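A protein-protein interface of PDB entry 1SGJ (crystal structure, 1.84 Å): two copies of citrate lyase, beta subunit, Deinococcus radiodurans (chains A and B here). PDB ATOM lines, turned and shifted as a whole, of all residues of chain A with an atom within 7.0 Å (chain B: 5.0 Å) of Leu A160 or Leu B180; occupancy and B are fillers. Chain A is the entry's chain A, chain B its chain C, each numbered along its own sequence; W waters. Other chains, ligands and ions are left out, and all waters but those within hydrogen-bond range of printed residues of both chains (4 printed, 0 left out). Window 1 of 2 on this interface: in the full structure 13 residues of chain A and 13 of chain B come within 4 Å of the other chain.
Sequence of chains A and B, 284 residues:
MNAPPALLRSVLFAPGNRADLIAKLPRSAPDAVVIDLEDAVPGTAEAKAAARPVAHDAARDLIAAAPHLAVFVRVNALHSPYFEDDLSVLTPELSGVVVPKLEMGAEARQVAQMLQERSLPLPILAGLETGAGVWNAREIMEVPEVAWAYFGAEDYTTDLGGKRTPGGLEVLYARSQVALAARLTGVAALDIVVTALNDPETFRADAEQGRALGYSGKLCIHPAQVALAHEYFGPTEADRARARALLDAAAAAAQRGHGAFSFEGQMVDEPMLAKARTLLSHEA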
ATOM      1  N   THR A 130     -17.268  -4.114 -13.394  1.00  0.00           N
ATOM      2  CA  THR A 130     -17.427  -3.054 -12.413  1.00  0.00           C
ATOM      3  C   THR A 130     -18.660  -3.450 -11.618  1.00  0.00           C
ATOM      4  O   THR A 130     -19.390  -4.349 -12.022  1.00  0.00           O
ATOM      5  CB  THR A 130     -17.681  -1.679 -13.058  1.00  0.00           C
ATOM      6  OG1 THR A 130     -18.922  -1.712 -13.765  1.00  0.00           O
ATOM      7  CG2 THR A 130     -16.563  -1.315 -14.015  1.00  0.00           C
ATOM      8  N   GLY A 131     -18.889  -2.790 -10.489  1.00  0.00           N
ATOM      9  CA  GLY A 131     -20.058  -3.101  -9.684  1.00  0.00           C
ATOM     10  C   GLY A 131     -21.354  -3.050 -10.473  1.00  0.00           C
ATOM     11  O   GLY A 131     -22.144  -3.989 -10.434  1.00  0.00           O
ATOM     12  N   ALA A 132     -21.575  -1.960 -11.205  1.00  0.00           N
ATOM     13  CA  ALA A 132     -22.799  -1.813 -11.987  1.00  0.00           C
ATOM     14  C   ALA A 132     -22.908  -2.863 -13.094  1.00  0.00           C
ATOM     15  O   ALA A 132     -23.991  -3.354 -13.380  1.00  0.00           O
ATOM     16  CB  ALA A 132     -22.877  -0.402 -12.586  1.00  0.00           C
ATOM     17  N   GLY A 133     -21.784  -3.203 -13.719  1.00  0.00           N
ATOM     18  CA  GLY A 133     -21.824  -4.202 -14.773  1.00  0.00           C
ATOM     19  C   GLY A 133     -22.344  -5.534 -14.249  1.00  0.00           C
ATOM     20  O   GLY A 133     -23.144  -6.203 -14.916  1.00  0.00           O
ATOM     21  N   VAL A 134     -21.894  -5.920 -13.056  1.00  0.00           N
ATOM     22  CA  VAL A 134     -22.327  -7.184 -12.446  1.00  0.00           C
ATOM     23  C   VAL A 134     -23.772  -7.084 -11.965  1.00  0.00           C
ATOM     24  O   VAL A 134     -24.584  -7.991 -12.185  1.00  0.00           O
ATOM     25  CB  VAL A 134     -21.410  -7.578 -11.253  1.00  0.00           C
ATOM     26  CG1 VAL A 134     -22.023  -8.744 -10.475  1.00  0.00           C
ATOM     27  CG2 VAL A 134     -20.025  -7.971 -11.770  1.00  0.00           C
ATOM     28  N   TRP A 135     -24.100  -5.969 -11.319  1.00  0.00           N
ATOM     29  CA  TRP A 135     -25.449  -5.761 -10.813  1.00  0.00           C
ATOM     30  C   TRP A 135     -26.472  -5.833 -11.944  1.00  0.00           C
ATOM     31  O   TRP A 135     -27.518  -6.462 -11.804  1.00  0.00           O
ATOM     32  CB  TRP A 135     -25.535  -4.405 -10.111  1.00  0.00           C
ATOM     33  CG  TRP A 135     -26.789  -4.209  -9.321  1.00  0.00           C
ATOM     34  CD1 TRP A 135     -27.981  -3.731  -9.773  1.00  0.00           C
ATOM     35  CD2 TRP A 135     -26.975  -4.512  -7.934  1.00  0.00           C
ATOM     36  NE1 TRP A 135     -28.904  -3.716  -8.750  1.00  0.00           N
ATOM     37  CE2 TRP A 135     -28.312  -4.195  -7.610  1.00  0.00           C
ATOM     38  CE3 TRP A 135     -26.142  -5.027  -6.934  1.00  0.00           C
ATOM     39  CZ2 TRP A 135     -28.834  -4.372  -6.330  1.00  0.00           C
ATOM     40  CZ3 TRP A 135     -26.658  -5.202  -5.661  1.00  0.00           C
ATOM     41  CH2 TRP A 135     -27.996  -4.876  -5.370  1.00  0.00           C
ATOM     42  N   ASP A 155     -10.772  -5.397 -12.697  1.00  0.00           N
ATOM     43  CA  ASP A 155     -11.436  -4.104 -12.623  1.00  0.00           C
ATOM     44  C   ASP A 155     -12.602  -4.108 -11.639  1.00  0.00           C
ATOM     45  O   ASP A 155     -12.947  -3.062 -11.090  1.00  0.00           O
ATOM     46  CB  ASP A 155     -11.917  -3.664 -14.004  1.00  0.00           C
ATOM     47  CG  ASP A 155     -10.794  -3.104 -14.864  1.00  0.00           C
ATOM     48  OD1 ASP A 155      -9.621  -3.141 -14.433  1.00  0.00           O
ATOM     49  OD2 ASP A 155     -11.086  -2.624 -15.975  1.00  0.00           O
ATOM     50  N   TYR A 156     -13.208  -5.275 -11.420  1.00  0.00           N
ATOM     51  CA  TYR A 156     -14.323  -5.387 -10.480  1.00  0.00           C
ATOM     52  C   TYR A 156     -13.861  -5.042  -9.073  1.00  0.00           C
ATOM     53  O   TYR A 156     -14.462  -4.197  -8.399  1.00  0.00           O
ATOM     54  CB  TYR A 156     -14.892  -6.810 -10.455  1.00  0.00           C
ATOM     55  CG  TYR A 156     -16.068  -6.976  -9.511  1.00  0.00           C
ATOM     56  CD1 TYR A 156     -17.338  -6.519  -9.866  1.00  0.00           C
ATOM     57  CD2 TYR A 156     -15.913  -7.590  -8.260  1.00  0.00           C
ATOM     58  CE1 TYR A 156     -18.422  -6.669  -9.010  1.00  0.00           C
ATOM     59  CE2 TYR A 156     -16.999  -7.743  -7.390  1.00  0.00           C
ATOM     60  CZ  TYR A 156     -18.248  -7.281  -7.775  1.00  0.00           C
ATOM     61  OH  TYR A 156     -19.332  -7.430  -6.944  1.00  0.00           O
ATOM     62  N   THR A 157     -12.799  -5.707  -8.624  1.00  0.00           N
ATOM     63  CA  THR A 157     -12.274  -5.468  -7.287  1.00  0.00           C
ATOM     64  C   THR A 157     -11.747  -4.043  -7.137  1.00  0.00           C
ATOM     65  O   THR A 157     -11.884  -3.437  -6.074  1.00  0.00           O
ATOM     66  CB  THR A 157     -11.157  -6.481  -6.920  1.00  0.00           C
ATOM     67  OG1 THR A 157     -10.142  -6.468  -7.932  1.00  0.00           O
ATOM     68  CG2 THR A 157     -11.734  -7.891  -6.802  1.00  0.00           C
ATOM     69  N   THR A 158     -11.146  -3.503  -8.194  1.00  0.00           N
ATOM     70  CA  THR A 158     -10.636  -2.137  -8.132  1.00  0.00           C
ATOM     71  C   THR A 158     -11.821  -1.199  -7.952  1.00  0.00           C
ATOM     72  O   THR A 158     -11.771  -0.249  -7.166  1.00  0.00           O
ATOM     73  CB  THR A 158      -9.889  -1.748  -9.427  1.00  0.00           C
ATOM     74  OG1 THR A 158      -8.685  -2.513  -9.531  1.00  0.00           O
ATOM     75  CG2 THR A 158      -9.541  -0.265  -9.419  1.00  0.00           C
ATOM     76  N   ASP A 159     -12.898  -1.481  -8.672  1.00  0.00           N
ATOM     77  CA  ASP A 159     -14.084  -0.652  -8.587  1.00  0.00           C
ATOM     78  C   ASP A 159     -14.711  -0.675  -7.194  1.00  0.00           C
ATOM     79  O   ASP A 159     -15.187   0.348  -6.719  1.00  0.00           O
ATOM     80  CB  ASP A 159     -15.112  -1.096  -9.626  1.00  0.00           C
ATOM     81  CG  ASP A 159     -16.271  -0.142  -9.728  1.00  0.00           C
ATOM     82  OD1 ASP A 159     -16.021   1.058  -9.954  1.00  0.00           O
ATOM     83  OD2 ASP A 159     -17.430  -0.585  -9.591  1.00  0.00           O
ATOM     84  N   LEU A 160     -14.712  -1.836  -6.540  1.00  0.00           N
ATOM     85  CA  LEU A 160     -15.295  -1.947  -5.203  1.00  0.00           C
ATOM     86  C   LEU A 160     -14.318  -1.615  -4.076  1.00  0.00           C
ATOM     87  O   LEU A 160     -14.696  -1.623  -2.909  1.00  0.00           O
ATOM     88  CB  LEU A 160     -15.869  -3.357  -4.971  1.00  0.00           C
ATOM     89  CG  LEU A 160     -17.353  -3.559  -5.309  1.00  0.00           C
ATOM     90  CD1 LEU A 160     -17.578  -3.340  -6.805  1.00  0.00           C
ATOM     91  CD2 LEU A 160     -17.795  -4.949  -4.899  1.00  0.00           C
ATOM     92  N   GLY A 161     -13.068  -1.327  -4.421  1.00  0.00           N
ATOM     93  CA  GLY A 161     -12.083  -1.009  -3.400  1.00  0.00           C
ATOM     94  C   GLY A 161     -11.597  -2.276  -2.721  1.00  0.00           C
ATOM     95  O   GLY A 161     -11.090  -2.252  -1.591  1.00  0.00           O
ATOM     96  N   GLY A 162     -11.755  -3.391  -3.430  1.00  0.00           N
ATOM     97  CA  GLY A 162     -11.353  -4.680  -2.910  1.00  0.00           C
ATOM     98  C   GLY A 162      -9.925  -5.046  -3.246  1.00  0.00           C
ATOM     99  O   GLY A 162      -9.128  -4.200  -3.649  1.00  0.00           O
ATOM    100  N   LYS A 163      -9.604  -6.321  -3.081  1.00  0.00           N
ATOM    101  CA  LYS A 163      -8.268  -6.819  -3.354  1.00  0.00           C
ATOM    102  C   LYS A 163      -8.401  -8.270  -3.825  1.00  0.00           C
ATOM    103  O   LYS A 163      -9.205  -9.032  -3.293  1.00  0.00           O
ATOM    104  CB  LYS A 163      -7.429  -6.732  -2.076  1.00  0.00           C
ATOM    105  CG  LYS A 163      -5.931  -6.842  -2.292  1.00  0.00           C
ATOM    106  CD  LYS A 163      -5.166  -6.542  -1.007  1.00  0.00           C
ATOM    107  CE  LYS A 163      -5.470  -5.135  -0.497  1.00  0.00           C
ATOM    108  NZ  LYS A 163      -4.776  -4.830   0.792  1.00  0.00           N
ATOM    109  N   GLU A 170     -13.369 -13.552  -2.982  1.00  0.00           N
ATOM    110  CA  GLU A 170     -13.846 -12.176  -2.990  1.00  0.00           C
ATOM    111  C   GLU A 170     -14.626 -11.807  -4.254  1.00  0.00           C
ATOM    112  O   GLU A 170     -15.280 -10.774  -4.291  1.00  0.00           O
ATOM    113  CB  GLU A 170     -12.683 -11.191  -2.781  1.00  0.00           C
ATOM    114  CG  GLU A 170     -11.765 -10.963  -3.977  1.00  0.00           C
ATOM    115  CD  GLU A 170     -10.797 -12.104  -4.228  1.00  0.00           C
ATOM    116  OE1 GLU A 170     -10.592 -12.936  -3.319  1.00  0.00           O
ATOM    117  OE2 GLU A 170     -10.226 -12.158  -5.341  1.00  0.00           O
ATOM    118  N   TYR A 173     -19.163 -14.360  -5.661  1.00  0.00           N
ATOM    119  CA  TYR A 173     -20.542 -13.908  -5.804  1.00  0.00           C
ATOM    120  C   TYR A 173     -20.735 -13.347  -7.220  1.00  0.00           C
ATOM    121  O   TYR A 173     -21.624 -13.764  -7.948  1.00  0.00           O
ATOM    122  CB  TYR A 173     -20.815 -12.829  -4.755  1.00  0.00           C
ATOM    123  CG  TYR A 173     -22.105 -12.062  -4.927  1.00  0.00           C
ATOM    124  CD1 TYR A 173     -23.286 -12.501  -4.339  1.00  0.00           C
ATOM    125  CD2 TYR A 173     -22.132 -10.868  -5.654  1.00  0.00           C
ATOM    126  CE1 TYR A 173     -24.474 -11.769  -4.458  1.00  0.00           C
ATOM    127  CE2 TYR A 173     -23.308 -10.130  -5.787  1.00  0.00           C
ATOM    128  CZ  TYR A 173     -24.474 -10.584  -5.183  1.00  0.00           C
ATOM    129  OH  TYR A 173     -25.633  -9.851  -5.291  1.00  0.00           O
ATOM    130  N   ALA A 174     -19.872 -12.410  -7.600  1.00  0.00           N
ATOM    131  CA  ALA A 174     -19.930 -11.781  -8.916  1.00  0.00           C
ATOM    132  C   ALA A 174     -19.728 -12.787 -10.060  1.00  0.00           C
ATOM    133  O   ALA A 174     -20.496 -12.811 -11.025  1.00  0.00           O
ATOM    134  CB  ALA A 174     -18.876 -10.678  -8.998  1.00  0.00           C
ATOM    135  N   GLN A 177     -22.860 -14.837 -10.488  1.00  0.00           N
ATOM    136  CA  GLN A 177     -23.991 -14.078 -11.007  1.00  0.00           C
ATOM    137  C   GLN A 177     -23.871 -13.886 -12.512  1.00  0.00           C
ATOM    138  O   GLN A 177     -24.838 -14.044 -13.237  1.00  0.00           O
ATOM    139  CB  GLN A 177     -24.089 -12.712 -10.322  1.00  0.00           C
ATOM    140  CG  GLN A 177     -25.293 -11.910 -10.786  1.00  0.00           C
ATOM    141  CD  GLN A 177     -25.765 -10.890  -9.774  1.00  0.00           C
ATOM    142  OE1 GLN A 177     -25.680  -9.676 -10.004  1.00  0.00           O
ATOM    143  NE2 GLN A 177     -26.270 -11.371  -8.651  1.00  0.00           N
ATOM    144  N   SER B 176     -20.891 -10.325   0.260  1.00  0.00           N
ATOM    145  CA  SER B 176     -20.519  -9.840  -1.063  1.00  0.00           C
ATOM    146  C   SER B 176     -21.580  -8.894  -1.612  1.00  0.00           C
ATOM    147  O   SER B 176     -21.261  -7.879  -2.238  1.00  0.00           O
ATOM    148  CB  SER B 176     -20.329 -11.018  -2.030  1.00  0.00           C
ATOM    149  OG  SER B 176     -19.304 -11.888  -1.582  1.00  0.00           O
ATOM    150  N   GLN B 177     -22.844  -9.223  -1.367  1.00  0.00           N
ATOM    151  CA  GLN B 177     -23.950  -8.405  -1.851  1.00  0.00           C
ATOM    152  C   GLN B 177     -23.991  -7.038  -1.176  1.00  0.00           C
ATOM    153  O   GLN B 177     -24.264  -6.029  -1.829  1.00  0.00           O
ATOM    154  CB  GLN B 177     -25.286  -9.121  -1.639  1.00  0.00           C
ATOM    155  CG  GLN B 177     -26.469  -8.363  -2.228  1.00  0.00           C
ATOM    156  CD  GLN B 177     -27.665  -9.251  -2.489  1.00  0.00           C
ATOM    157  OE1 GLN B 177     -28.667  -9.208  -1.765  1.00  0.00           O
ATOM    158  NE2 GLN B 177     -27.565 -10.068  -3.522  1.00  0.00           N
ATOM    159  N   VAL B 178     -23.731  -7.000   0.128  1.00  0.00           N
ATOM    160  CA  VAL B 178     -23.741  -5.725   0.840  1.00  0.00           C
ATOM    161  C   VAL B 178     -22.602  -4.827   0.341  1.00  0.00           C
ATOM    162  O   VAL B 178     -22.794  -3.629   0.138  1.00  0.00           O
ATOM    163  CB  VAL B 178     -23.620  -5.930   2.370  1.00  0.00           C
ATOM    164  CG1 VAL B 178     -23.320  -4.601   3.062  1.00  0.00           C
ATOM    165  CG2 VAL B 178     -24.923  -6.485   2.912  1.00  0.00           C
ATOM    166  N   ALA B 179     -21.423  -5.413   0.136  1.00  0.00           N
ATOM    167  CA  ALA B 179     -20.264  -4.660  -0.352  1.00  0.00           C
ATOM    168  C   ALA B 179     -20.552  -4.032  -1.721  1.00  0.00           C
ATOM    169  O   ALA B 179     -20.203  -2.876  -1.977  1.00  0.00           O
ATOM    170  CB  ALA B 179     -19.059  -5.577  -0.459  1.00  0.00           C
ATOM    171  N   LEU B 180     -21.185  -4.811  -2.593  1.00  0.00           N
ATOM    172  CA  LEU B 180     -21.529  -4.365  -3.937  1.00  0.00           C
ATOM    173  C   LEU B 180     -22.590  -3.269  -3.904  1.00  0.00           C
ATOM    174  O   LEU B 180     -22.482  -2.268  -4.619  1.00  0.00           O
ATOM    175  CB  LEU B 180     -22.030  -5.547  -4.775  1.00  0.00           C
ATOM    176  CG  LEU B 180     -22.501  -5.203  -6.193  1.00  0.00           C
ATOM    177  CD1 LEU B 180     -21.394  -4.465  -6.942  1.00  0.00           C
ATOM    178  CD2 LEU B 180     -22.892  -6.480  -6.935  1.00  0.00           C
ATOM    179  N   ALA B 181     -23.615  -3.457  -3.078  1.00  0.00           N
ATOM    180  CA  ALA B 181     -24.680  -2.470  -2.966  1.00  0.00           C
ATOM    181  C   ALA B 181     -24.127  -1.173  -2.365  1.00  0.00           C
ATOM    182  O   ALA B 181     -24.544  -0.073  -2.731  1.00  0.00           O
ATOM    183  CB  ALA B 181     -25.810  -3.019  -2.102  1.00  0.00           C
ATOM    184  N   ALA B 182     -23.180  -1.300  -1.446  1.00  0.00           N
ATOM    185  CA  ALA B 182     -22.597  -0.114  -0.827  1.00  0.00           C
ATOM    186  C   ALA B 182     -21.857   0.707  -1.889  1.00  0.00           C
ATOM    187  O   ALA B 182     -21.956   1.940  -1.920  1.00  0.00           O
ATOM    188  CB  ALA B 182     -21.652  -0.515   0.274  1.00  0.00           C
ATOM    189  N   ARG B 183     -21.123   0.019  -2.760  1.00  0.00           N
ATOM    190  CA  ARG B 183     -20.384   0.682  -3.828  1.00  0.00           C
ATOM    191  C   ARG B 183     -21.308   1.440  -4.777  1.00  0.00           C
ATOM    192  O   ARG B 183     -21.041   2.588  -5.138  1.00  0.00           O
ATOM    193  CB  ARG B 183     -19.590  -0.337  -4.649  1.00  0.00           C
ATOM    194  CG  ARG B 183     -19.082   0.209  -5.984  1.00  0.00           C
ATOM    195  CD  ARG B 183     -18.121   1.388  -5.795  1.00  0.00           C
ATOM    196  NE  ARG B 183     -17.662   1.924  -7.078  1.00  0.00           N
ATOM    197  CZ  ARG B 183     -18.395   2.684  -7.888  1.00  0.00           C
ATOM    198  NH1 ARG B 183     -19.633   3.026  -7.554  1.00  0.00           N
ATOM    199  NH2 ARG B 183     -17.898   3.078  -9.056  1.00  0.00           N
ATOM    200  N   LEU B 184     -22.385   0.779  -5.183  1.00  0.00           N
ATOM    201  CA  LEU B 184     -23.352   1.352  -6.117  1.00  0.00           C
ATOM    202  C   LEU B 184     -24.125   2.551  -5.571  1.00  0.00           C
ATOM    203  O   LEU B 184     -24.664   3.347  -6.339  1.00  0.00           O
ATOM    204  CB  LEU B 184     -24.339   0.272  -6.557  1.00  0.00           C
ATOM    205  CG  LEU B 184     -23.771  -0.862  -7.418  1.00  0.00           C
ATOM    206  CD1 LEU B 184     -24.786  -1.979  -7.508  1.00  0.00           C
ATOM    207  CD2 LEU B 184     -23.421  -0.334  -8.802  1.00  0.00           C
ATOM    208  N   LEU B 213     -13.116  -8.083  -0.209  1.00  0.00           N
ATOM    209  CA  LEU B 213     -14.486  -7.939  -0.718  1.00  0.00           C
ATOM    210  C   LEU B 213     -14.961  -6.511  -0.987  1.00  0.00           C
ATOM    211  O   LEU B 213     -16.034  -6.313  -1.558  1.00  0.00           O
ATOM    212  CB  LEU B 213     -15.481  -8.598   0.245  1.00  0.00           C
ATOM    213  CG  LEU B 213     -15.588 -10.127   0.211  1.00  0.00           C
ATOM    214  CD1 LEU B 213     -16.292 -10.620   1.463  1.00  0.00           C
ATOM    215  CD2 LEU B 213     -16.348 -10.560  -1.029  1.00  0.00           C
ATOM    216  N   GLY B 214     -14.193  -5.516  -0.564  1.00  0.00           N
ATOM    217  CA  GLY B 214     -14.609  -4.146  -0.802  1.00  0.00           C
ATOM    218  C   GLY B 214     -15.046  -3.342   0.418  1.00  0.00           C
ATOM    219  O   GLY B 214     -15.479  -2.196   0.271  1.00  0.00           O
HETATM  220  O   HOH W   1     -14.668   0.083  -0.616  1.00  0.00           O
HETATM  221  O   HOH W   2     -19.153  -8.297  -4.393  1.00  0.00           O
HETATM  222  O   HOH W   3     -17.729 -12.997  -3.505  1.00  0.00           O
HETATM  223  O   HOH W   4     -16.493  -7.908  -3.789  1.00  0.00           O
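Leu B180 touches Gly A131. Leu B184 touches Gly A131 (CD2 to C, 3.8 Å). Ala A132 touches Leu B184. CE3 of Trp A135 touches CD2 of Leu B180, at 3.6 Å. CD2 of Trp A135 touches CD1 of Leu B184 (3.4 Å). Tyr A156 touches Leu B180 (OH to CD1, 3.6 Å). CD1 of Leu A160 touches CG of Arg B183, at 3.9 Å. Gly B214 touches Gly A162 (N to CA, 3.8 Å). Glu A170 touches Leu B213 (O to CD2, 3.4 Å). Tyr A173 touches Ser B176.
Position printed for both chains: 177. Of the 15 pairs that touch across the chains among the printed residues, none has its exchanged pair printed and touching as well.
Thr A157 touches none of the printed residues of chain B. Printed residues of chain B within 4 Å of Leu A160: Leu B180 (3.9 Å), Arg B183 (3.9 Å) and Gly B214 (3.3 Å). Of the printed residues of chain B, Gly A162 touches Gly B214. Of the printed residues of chain B, Glu A170 touches Leu B213. Of the printed residues of chain A, Gln B177 touches Tyr A173 (2.6 Å). Of the printed residues of chain A, Leu B180 touches Gly A131, Trp A135, Tyr A156, Leu A160 and Tyr A173. Of the printed residues of chain A, Leu B184 touches Gly A131 (3.8 Å), Ala A132 (3.4 Å) and Trp A135 (3.4 Å). The nearest printed residue of chain B that does not touch Leu A160 is Leu B213 (4.02 Å). The nearest residue of chain A that does not touch Leu B180 is Val A134 (4.3 Å).
Water W1 lies within hydrogen-bond range of O of Gly B214 and O of Leu A160. Water W2 lies within hydrogen-bond range of OH of Tyr A156 (2.7 Å) and O of Ser B176 (3.0 Å). Water W3 lies within hydrogen-bond range of OG of Ser B176 (2.7 Å), N of Tyr A173 (2.9 Å) and O of Glu A170 (3.4 Å). Water W4 lies within hydrogen-bond range of the backbone carbonyl oxygen (O) of Leu B213 (2.8 Å) and the backbone carbonyl oxygen (O) of Glu A170 (3.2 Å).
Hydrophobic or aromatic side chains of chain A that line the printed part of chain B: Ala A132, Trp A135, Tyr A156, Leu A160 and Tyr A173. Of the 11 printed residues of chain B, 7 touch a printed residue of chain A.
The side-chain carboxylate (OD2) of Asp A159 lies within hydrogen-bond range of the backbone NH (N) of Gly A131 (2.8 Å). The backbone NH (N) of Gly A162 lies within hydrogen-bond range of the backbone carbonyl oxygen (O) of Thr A157, 2.6 Å away.
The side-chain carboxylate of Asp A159 lies within salt-bridge range of the guanidinium group of Arg B183, 2.9 Å away. The side-chain amide nitrogen of Gln B177 is in hydrogen-bond range of the side-chain hydroxyl of Tyr A173. O of Gly B214 lies close to O of Leu A160 (3.3 Å).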
